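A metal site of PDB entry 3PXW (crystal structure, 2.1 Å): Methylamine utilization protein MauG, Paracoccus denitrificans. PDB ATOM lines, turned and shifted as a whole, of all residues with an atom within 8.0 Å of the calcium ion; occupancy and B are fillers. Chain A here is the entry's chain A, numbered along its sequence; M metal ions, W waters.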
ATOM      1  N   ARG A  39      11.888  14.548  34.816  1.00  0.00           N
ATOM      2  CA  ARG A  39      11.936  15.832  34.092  1.00  0.00           C
ATOM      3  C   ARG A  39      12.088  15.651  32.573  1.00  0.00           C
ATOM      4  O   ARG A  39      12.891  16.333  31.925  1.00  0.00           O
ATOM      5  CB  ARG A  39      13.024  16.757  34.649  1.00  0.00           C
ATOM      6  CG  ARG A  39      12.605  18.223  34.671  1.00  0.00           C
ATOM      7  CD  ARG A  39      13.698  19.144  35.177  1.00  0.00           C
ATOM      8  NE  ARG A  39      14.513  19.609  34.076  1.00  0.00           N
ATOM      9  CZ  ARG A  39      14.552  20.854  33.609  1.00  0.00           C
ATOM     10  NH1 ARG A  39      13.841  21.829  34.171  1.00  0.00           N
ATOM     11  NH2 ARG A  39      15.324  21.120  32.584  1.00  0.00           N
ATOM     12  N   THR A  42      15.670  14.975  31.182  1.00  0.00           N
ATOM     13  CA  THR A  42      16.623  16.077  31.246  1.00  0.00           C
ATOM     14  C   THR A  42      17.070  16.278  32.709  1.00  0.00           C
ATOM     15  O   THR A  42      16.627  15.550  33.603  1.00  0.00           O
ATOM     16  CB  THR A  42      16.048  17.406  30.683  1.00  0.00           C
ATOM     17  OG1 THR A  42      14.962  17.854  31.499  1.00  0.00           O
ATOM     18  CG2 THR A  42      15.570  17.230  29.252  1.00  0.00           C
ATOM     19  N   ASP A  43      17.926  17.271  32.928  1.00  0.00           N
ATOM     20  CA  ASP A  43      18.640  17.433  34.192  1.00  0.00           C
ATOM     21  C   ASP A  43      18.069  18.547  35.081  1.00  0.00           C
ATOM     22  O   ASP A  43      18.193  19.738  34.759  1.00  0.00           O
ATOM     23  CB  ASP A  43      20.139  17.677  33.924  1.00  0.00           C
ATOM     24  CG  ASP A  43      21.001  17.401  35.136  1.00  0.00           C
ATOM     25  OD1 ASP A  43      22.241  17.462  34.992  1.00  0.00           O
ATOM     26  OD2 ASP A  43      20.460  17.134  36.229  1.00  0.00           O
ATOM     27  N   LEU A  51      20.818  25.549  35.406  1.00  0.00           N
ATOM     28  CA  LEU A  51      20.382  24.333  34.747  1.00  0.00           C
ATOM     29  C   LEU A  51      20.920  24.229  33.304  1.00  0.00           C
ATOM     30  O   LEU A  51      20.583  23.285  32.576  1.00  0.00           O
ATOM     31  CB  LEU A  51      18.851  24.249  34.749  1.00  0.00           C
ATOM     32  CG  LEU A  51      18.058  23.567  35.881  1.00  0.00           C
ATOM     33  CD1 LEU A  51      18.582  23.866  37.271  1.00  0.00           C
ATOM     34  CD2 LEU A  51      16.572  23.941  35.786  1.00  0.00           C
ATOM     35  N   ALA A  52      21.773  25.188  32.911  1.00  0.00           N
ATOM     36  CA  ALA A  52      22.255  25.315  31.533  1.00  0.00           C
ATOM     37  C   ALA A  52      23.132  24.151  31.089  1.00  0.00           C
ATOM     38  O   ALA A  52      23.011  23.677  29.962  1.00  0.00           O
ATOM     39  CB  ALA A  52      22.989  26.637  31.331  1.00  0.00           C
ATOM     40  N   ASN A  66      23.857  21.986  26.885  1.00  0.00           N
ATOM     41  CA  ASN A  66      22.655  21.610  27.601  1.00  0.00           C
ATOM     42  C   ASN A  66      22.299  20.139  27.392  1.00  0.00           C
ATOM     43  O   ASN A  66      22.425  19.616  26.279  1.00  0.00           O
ATOM     44  CB  ASN A  66      21.496  22.505  27.152  1.00  0.00           C
ATOM     45  CG  ASN A  66      20.261  22.338  28.009  1.00  0.00           C
ATOM     46  OD1 ASN A  66      19.214  21.875  27.523  1.00  0.00           O
ATOM     47  ND2 ASN A  66      20.363  22.685  29.285  1.00  0.00           N
ATOM     48  N   THR A  67      21.906  19.464  28.464  1.00  0.00           N
ATOM     49  CA  THR A  67      21.454  18.072  28.387  1.00  0.00           C
ATOM     50  C   THR A  67      20.055  18.031  27.774  1.00  0.00           C
ATOM     51  O   THR A  67      19.098  18.533  28.371  1.00  0.00           O
ATOM     52  CB  THR A  67      21.454  17.404  29.785  1.00  0.00           C
ATOM     53  OG1 THR A  67      22.801  17.329  30.285  1.00  0.00           O
ATOM     54  CG2 THR A  67      20.900  15.988  29.704  1.00  0.00           C
ATOM     55  N   PRO A  68      19.927  17.446  26.574  1.00  0.00           N
ATOM     56  CA  PRO A  68      18.631  17.360  25.877  1.00  0.00           C
ATOM     57  C   PRO A  68      17.785  16.147  26.293  1.00  0.00           C
ATOM     58  O   PRO A  68      18.318  15.150  26.789  1.00  0.00           O
ATOM     59  CB  PRO A  68      19.053  17.194  24.421  1.00  0.00           C
ATOM     60  CG  PRO A  68      20.373  16.488  24.477  1.00  0.00           C
ATOM     61  CD  PRO A  68      20.994  16.777  25.822  1.00  0.00           C
ATOM     62  N   THR A  69      16.482  16.232  26.060  1.00  0.00           N
ATOM     63  CA  THR A  69      15.579  15.096  26.274  1.00  0.00           C
ATOM     64  C   THR A  69      15.938  13.868  25.440  1.00  0.00           C
ATOM     65  O   THR A  69      16.435  13.976  24.318  1.00  0.00           O
ATOM     66  CB  THR A  69      14.089  15.462  26.009  1.00  0.00           C
ATOM     67  OG1 THR A  69      13.272  14.326  26.279  1.00  0.00           O
ATOM     68  CG2 THR A  69      13.865  15.909  24.555  1.00  0.00           C
ATOM     69  N   TRP A  93      23.919  17.601  19.926  1.00  0.00           N
ATOM     70  CA  TRP A  93      23.610  18.897  19.319  1.00  0.00           C
ATOM     71  C   TRP A  93      24.415  19.125  18.041  1.00  0.00           C
ATOM     72  O   TRP A  93      23.937  19.793  17.124  1.00  0.00           O
ATOM     73  CB  TRP A  93      23.875  20.038  20.301  1.00  0.00           C
ATOM     74  CG  TRP A  93      22.938  20.140  21.470  1.00  0.00           C
ATOM     75  CD1 TRP A  93      23.155  19.698  22.739  1.00  0.00           C
ATOM     76  CD2 TRP A  93      21.646  20.766  21.485  1.00  0.00           C
ATOM     77  NE1 TRP A  93      22.085  19.991  23.549  1.00  0.00           N
ATOM     78  CE2 TRP A  93      21.140  20.652  22.808  1.00  0.00           C
ATOM     79  CE3 TRP A  93      20.873  21.414  20.520  1.00  0.00           C
ATOM     80  CZ2 TRP A  93      19.875  21.146  23.179  1.00  0.00           C
ATOM     81  CZ3 TRP A  93      19.621  21.923  20.903  1.00  0.00           C
ATOM     82  CH2 TRP A  93      19.140  21.781  22.221  1.00  0.00           C
ATOM     83  N   ASN A 271       7.777  18.137  24.495  1.00  0.00           N
ATOM     84  CA  ASN A 271       8.121  18.399  25.898  1.00  0.00           C
ATOM     85  C   ASN A 271       8.939  19.671  26.126  1.00  0.00           C
ATOM     86  O   ASN A 271       9.497  19.864  27.205  1.00  0.00           O
ATOM     87  CB  ASN A 271       8.815  17.195  26.525  1.00  0.00           C
ATOM     88  CG  ASN A 271       7.929  15.975  26.573  1.00  0.00           C
ATOM     89  OD1 ASN A 271       6.765  16.064  26.964  1.00  0.00           O
ATOM     90  ND2 ASN A 271       8.491  14.813  26.195  1.00  0.00           N
ATOM     91  N   VAL A 272       8.991  20.545  25.129  1.00  0.00           N
ATOM     92  CA  VAL A 272       9.784  21.776  25.229  1.00  0.00           C
ATOM     93  C   VAL A 272       9.373  22.634  26.446  1.00  0.00           C
ATOM     94  O   VAL A 272      10.229  23.265  27.090  1.00  0.00           O
ATOM     95  CB  VAL A 272       9.778  22.588  23.898  1.00  0.00           C
ATOM     96  CG1 VAL A 272       8.410  23.220  23.611  1.00  0.00           C
ATOM     97  CG2 VAL A 272      10.866  23.652  23.908  1.00  0.00           C
ATOM     98  N   VAL A 274       8.602  21.751  29.379  1.00  0.00           N
ATOM     99  CA  VAL A 274       9.147  21.243  30.644  1.00  0.00           C
ATOM    100  C   VAL A 274      10.656  20.936  30.629  1.00  0.00           C
ATOM    101  O   VAL A 274      11.196  20.398  31.597  1.00  0.00           O
ATOM    102  CB  VAL A 274       8.335  20.014  31.168  1.00  0.00           C
ATOM    103  CG1 VAL A 274       6.857  20.381  31.373  1.00  0.00           C
ATOM    104  CG2 VAL A 274       8.468  18.822  30.227  1.00  0.00           C
ATOM    105  N   THR A 275      11.341  21.286  29.535  1.00  0.00           N
ATOM    106  CA  THR A 275      12.767  20.958  29.366  1.00  0.00           C
ATOM    107  C   THR A 275      13.708  22.180  29.280  1.00  0.00           C
ATOM    108  O   THR A 275      14.738  22.141  28.601  1.00  0.00           O
ATOM    109  CB  THR A 275      13.023  20.059  28.123  1.00  0.00           C
ATOM    110  OG1 THR A 275      12.521  20.711  26.958  1.00  0.00           O
ATOM    111  CG2 THR A 275      12.361  18.700  28.287  1.00  0.00           C
ATOM    112  N   GLY A 276      13.334  23.263  29.963  1.00  0.00           N
ATOM    113  CA  GLY A 276      14.171  24.459  30.047  1.00  0.00           C
ATOM    114  C   GLY A 276      15.414  24.185  30.872  1.00  0.00           C
ATOM    115  O   GLY A 276      15.416  23.258  31.685  1.00  0.00           O
ATOM    116  N   PRO A 277      16.480  24.990  30.701  1.00  0.00           N
ATOM    117  CA  PRO A 277      16.583  26.137  29.806  1.00  0.00           C
ATOM    118  C   PRO A 277      16.805  25.724  28.334  1.00  0.00           C
ATOM    119  O   PRO A 277      16.940  24.527  28.036  1.00  0.00           O
ATOM    120  CB  PRO A 277      17.768  26.921  30.368  1.00  0.00           C
ATOM    121  CG  PRO A 277      18.619  25.913  31.040  1.00  0.00           C
ATOM    122  CD  PRO A 277      17.706  24.802  31.488  1.00  0.00           C
ATOM    123  N   TYR A 278      16.860  26.700  27.445  1.00  0.00           N
ATOM    124  CA  TYR A 278      16.727  26.387  26.019  1.00  0.00           C
ATOM    125  C   TYR A 278      17.991  26.613  25.206  1.00  0.00           C
ATOM    126  O   TYR A 278      18.878  27.338  25.634  1.00  0.00           O
ATOM    127  CB  TYR A 278      15.496  27.101  25.438  1.00  0.00           C
ATOM    128  CG  TYR A 278      14.265  26.689  26.194  1.00  0.00           C
ATOM    129  CD1 TYR A 278      13.738  27.488  27.195  1.00  0.00           C
ATOM    130  CD2 TYR A 278      13.688  25.443  25.959  1.00  0.00           C
ATOM    131  CE1 TYR A 278      12.635  27.088  27.923  1.00  0.00           C
ATOM    132  CE2 TYR A 278      12.591  25.030  26.687  1.00  0.00           C
ATOM    133  CZ  TYR A 278      12.063  25.852  27.654  1.00  0.00           C
ATOM    134  OH  TYR A 278      10.973  25.435  28.362  1.00  0.00           O
ATOM    135  N   MET A 279      18.025  25.978  24.037  1.00  0.00           N
ATOM    136  CA  MET A 279      19.158  26.027  23.092  1.00  0.00           C
ATOM    137  C   MET A 279      20.328  25.138  23.529  1.00  0.00           C
ATOM    138  O   MET A 279      20.318  24.578  24.630  1.00  0.00           O
ATOM    139  CB  MET A 279      19.605  27.475  22.816  1.00  0.00           C
ATOM    140  CG  MET A 279      18.465  28.432  22.401  1.00  0.00           C
ATOM    141  SD  MET A 279      17.595  27.881  20.916  1.00  0.00           S
ATOM    142  CE  MET A 279      16.177  28.970  20.904  1.00  0.00           C
ATOM    143  N   HIS A 280      21.323  25.022  22.657  1.00  0.00           N
ATOM    144  CA  HIS A 280      22.414  24.061  22.812  1.00  0.00           C
ATOM    145  C   HIS A 280      23.265  24.341  24.042  1.00  0.00           C
ATOM    146  O   HIS A 280      23.883  23.429  24.583  1.00  0.00           O
ATOM    147  CB  HIS A 280      23.286  23.984  21.552  1.00  0.00           C
ATOM    148  CG  HIS A 280      24.037  25.238  21.243  1.00  0.00           C
ATOM    149  ND1 HIS A 280      23.571  26.184  20.354  1.00  0.00           N
ATOM    150  CD2 HIS A 280      25.229  25.707  21.690  1.00  0.00           C
ATOM    151  CE1 HIS A 280      24.438  27.185  20.284  1.00  0.00           C
ATOM    152  NE2 HIS A 280      25.452  26.914  21.071  1.00  0.00           N
ATOM    153  N   ASN A 281      23.268  25.592  24.488  1.00  0.00           N
ATOM    154  CA  ASN A 281      24.024  26.040  25.664  1.00  0.00           C
ATOM    155  C   ASN A 281      23.137  26.475  26.839  1.00  0.00           C
ATOM    156  O   ASN A 281      23.624  27.065  27.809  1.00  0.00           O
ATOM    157  CB  ASN A 281      24.986  27.173  25.288  1.00  0.00           C
ATOM    158  CG  ASN A 281      24.288  28.329  24.596  1.00  0.00           C
ATOM    159  OD1 ASN A 281      23.064  28.456  24.657  1.00  0.00           O
ATOM    160  ND2 ASN A 281      25.058  29.167  23.930  1.00  0.00           N
ATOM    161  N   GLY A 282      21.840  26.180  26.761  1.00  0.00           N
ATOM    162  CA  GLY A 282      20.884  26.492  27.818  1.00  0.00           C
ATOM    163  C   GLY A 282      20.837  27.955  28.218  1.00  0.00           C
ATOM    164  O   GLY A 282      20.557  28.274  29.366  1.00  0.00           O
ATOM    165  N   VAL A 283      21.122  28.843  27.262  1.00  0.00           N
ATOM    166  CA  VAL A 283      21.233  30.286  27.536  1.00  0.00           C
ATOM    167  C   VAL A 283      19.932  30.942  28.013  1.00  0.00           C
ATOM    168  O   VAL A 283      19.964  31.853  28.827  1.00  0.00           O
ATOM    169  CB  VAL A 283      21.877  31.039  26.334  1.00  0.00           C
ATOM    170  CG1 VAL A 283      20.956  31.015  25.096  1.00  0.00           C
ATOM    171  CG2 VAL A 283      22.286  32.471  26.697  1.00  0.00           C
ATOM    172  N   PHE A 284      18.788  30.481  27.505  1.00  0.00           N
ATOM    173  CA  PHE A 284      17.494  31.048  27.900  1.00  0.00           C
ATOM    174  C   PHE A 284      16.714  30.125  28.817  1.00  0.00           C
ATOM    175  O   PHE A 284      16.392  28.998  28.451  1.00  0.00           O
ATOM    176  CB  PHE A 284      16.634  31.379  26.673  1.00  0.00           C
ATOM    177  CG  PHE A 284      17.356  32.151  25.608  1.00  0.00           C
ATOM    178  CD1 PHE A 284      18.102  33.279  25.919  1.00  0.00           C
ATOM    179  CD2 PHE A 284      17.281  31.755  24.273  1.00  0.00           C
ATOM    180  CE1 PHE A 284      18.773  33.988  24.929  1.00  0.00           C
ATOM    181  CE2 PHE A 284      17.937  32.449  23.286  1.00  0.00           C
ATOM    182  CZ  PHE A 284      18.692  33.574  23.606  1.00  0.00           C
ATOM    183  N   THR A 285      16.369  30.640  29.995  1.00  0.00           N
ATOM    184  CA  THR A 285      15.624  29.866  30.989  1.00  0.00           C
ATOM    185  C   THR A 285      14.146  29.661  30.602  1.00  0.00           C
ATOM    186  O   THR A 285      13.573  28.600  30.814  1.00  0.00           O
ATOM    187  CB  THR A 285      15.709  30.515  32.399  1.00  0.00           C
ATOM    188  OG1 THR A 285      14.993  31.750  32.399  1.00  0.00           O
ATOM    189  CG2 THR A 285      17.159  30.776  32.794  1.00  0.00           C
HETATM  190 CA    CA M   1      16.877  22.244  27.508  1.00  0.00          CA
HETATM  191  O   HOH W   1      16.882  19.904  27.273  1.00  0.00           O
HETATM  192  O   HOH W   2      17.432  21.760  29.975  1.00  0.00           O
HETATM  193  O   HOH W   3      17.533  22.825  25.265  1.00  0.00           O
HETATM  194  O   HOH W   4      14.848  22.006  25.915  1.00  0.00           O
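The side-chain amide nitrogen (ND2) of Asn 66 is in hydrogen-bond range of the backbone carbonyl oxygen (O) of Leu 51, at 3.4 Å. The backbone carbonyl oxygen (O) of Ala 52 sits at hydrogen-bond distance from the side-chain amide nitrogen (ND2) of Asn 66, at 2.9 Å. The backbone carbonyl oxygen (O) of His 280 sits at hydrogen-bond distance from the backbone NH (N) of Asn 66. The side-chain hydroxyl (OG1) of Thr 275 lies within hydrogen-bond range of the backbone carbonyl oxygen (O) of Asn 271, at 3.2 Å. NE1 of Trp 93 lies within hydrogen-bond range of O of Asn 66, at 2.8 Å. The side-chain hydroxyl (OG1) of Thr 275 lies close to the backbone carbonyl oxygen (O) of Val 272 (3.4 Å).
The nearest printed residue that does not touch the calcium ion is Gly 276 (4.2 Å).
The calcium ion is bound by O of Pro 277 (2.3 Å), water W1 (2.4 Å), OD1 of Asn 66 (2.4 Å), O of Thr 275 (2.4 Å), water W3 (2.4 Å), water W2 (2.6 Å) and water W4 (2.6 Å). The calcium ion has seven donor atoms within binding distance.
Water W2 lies within hydrogen-bond range of O of Gly 276 (3.0 Å), ND2 of Asn 66 (3.1 Å) and NH2 of Arg 39 (3.4 Å).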
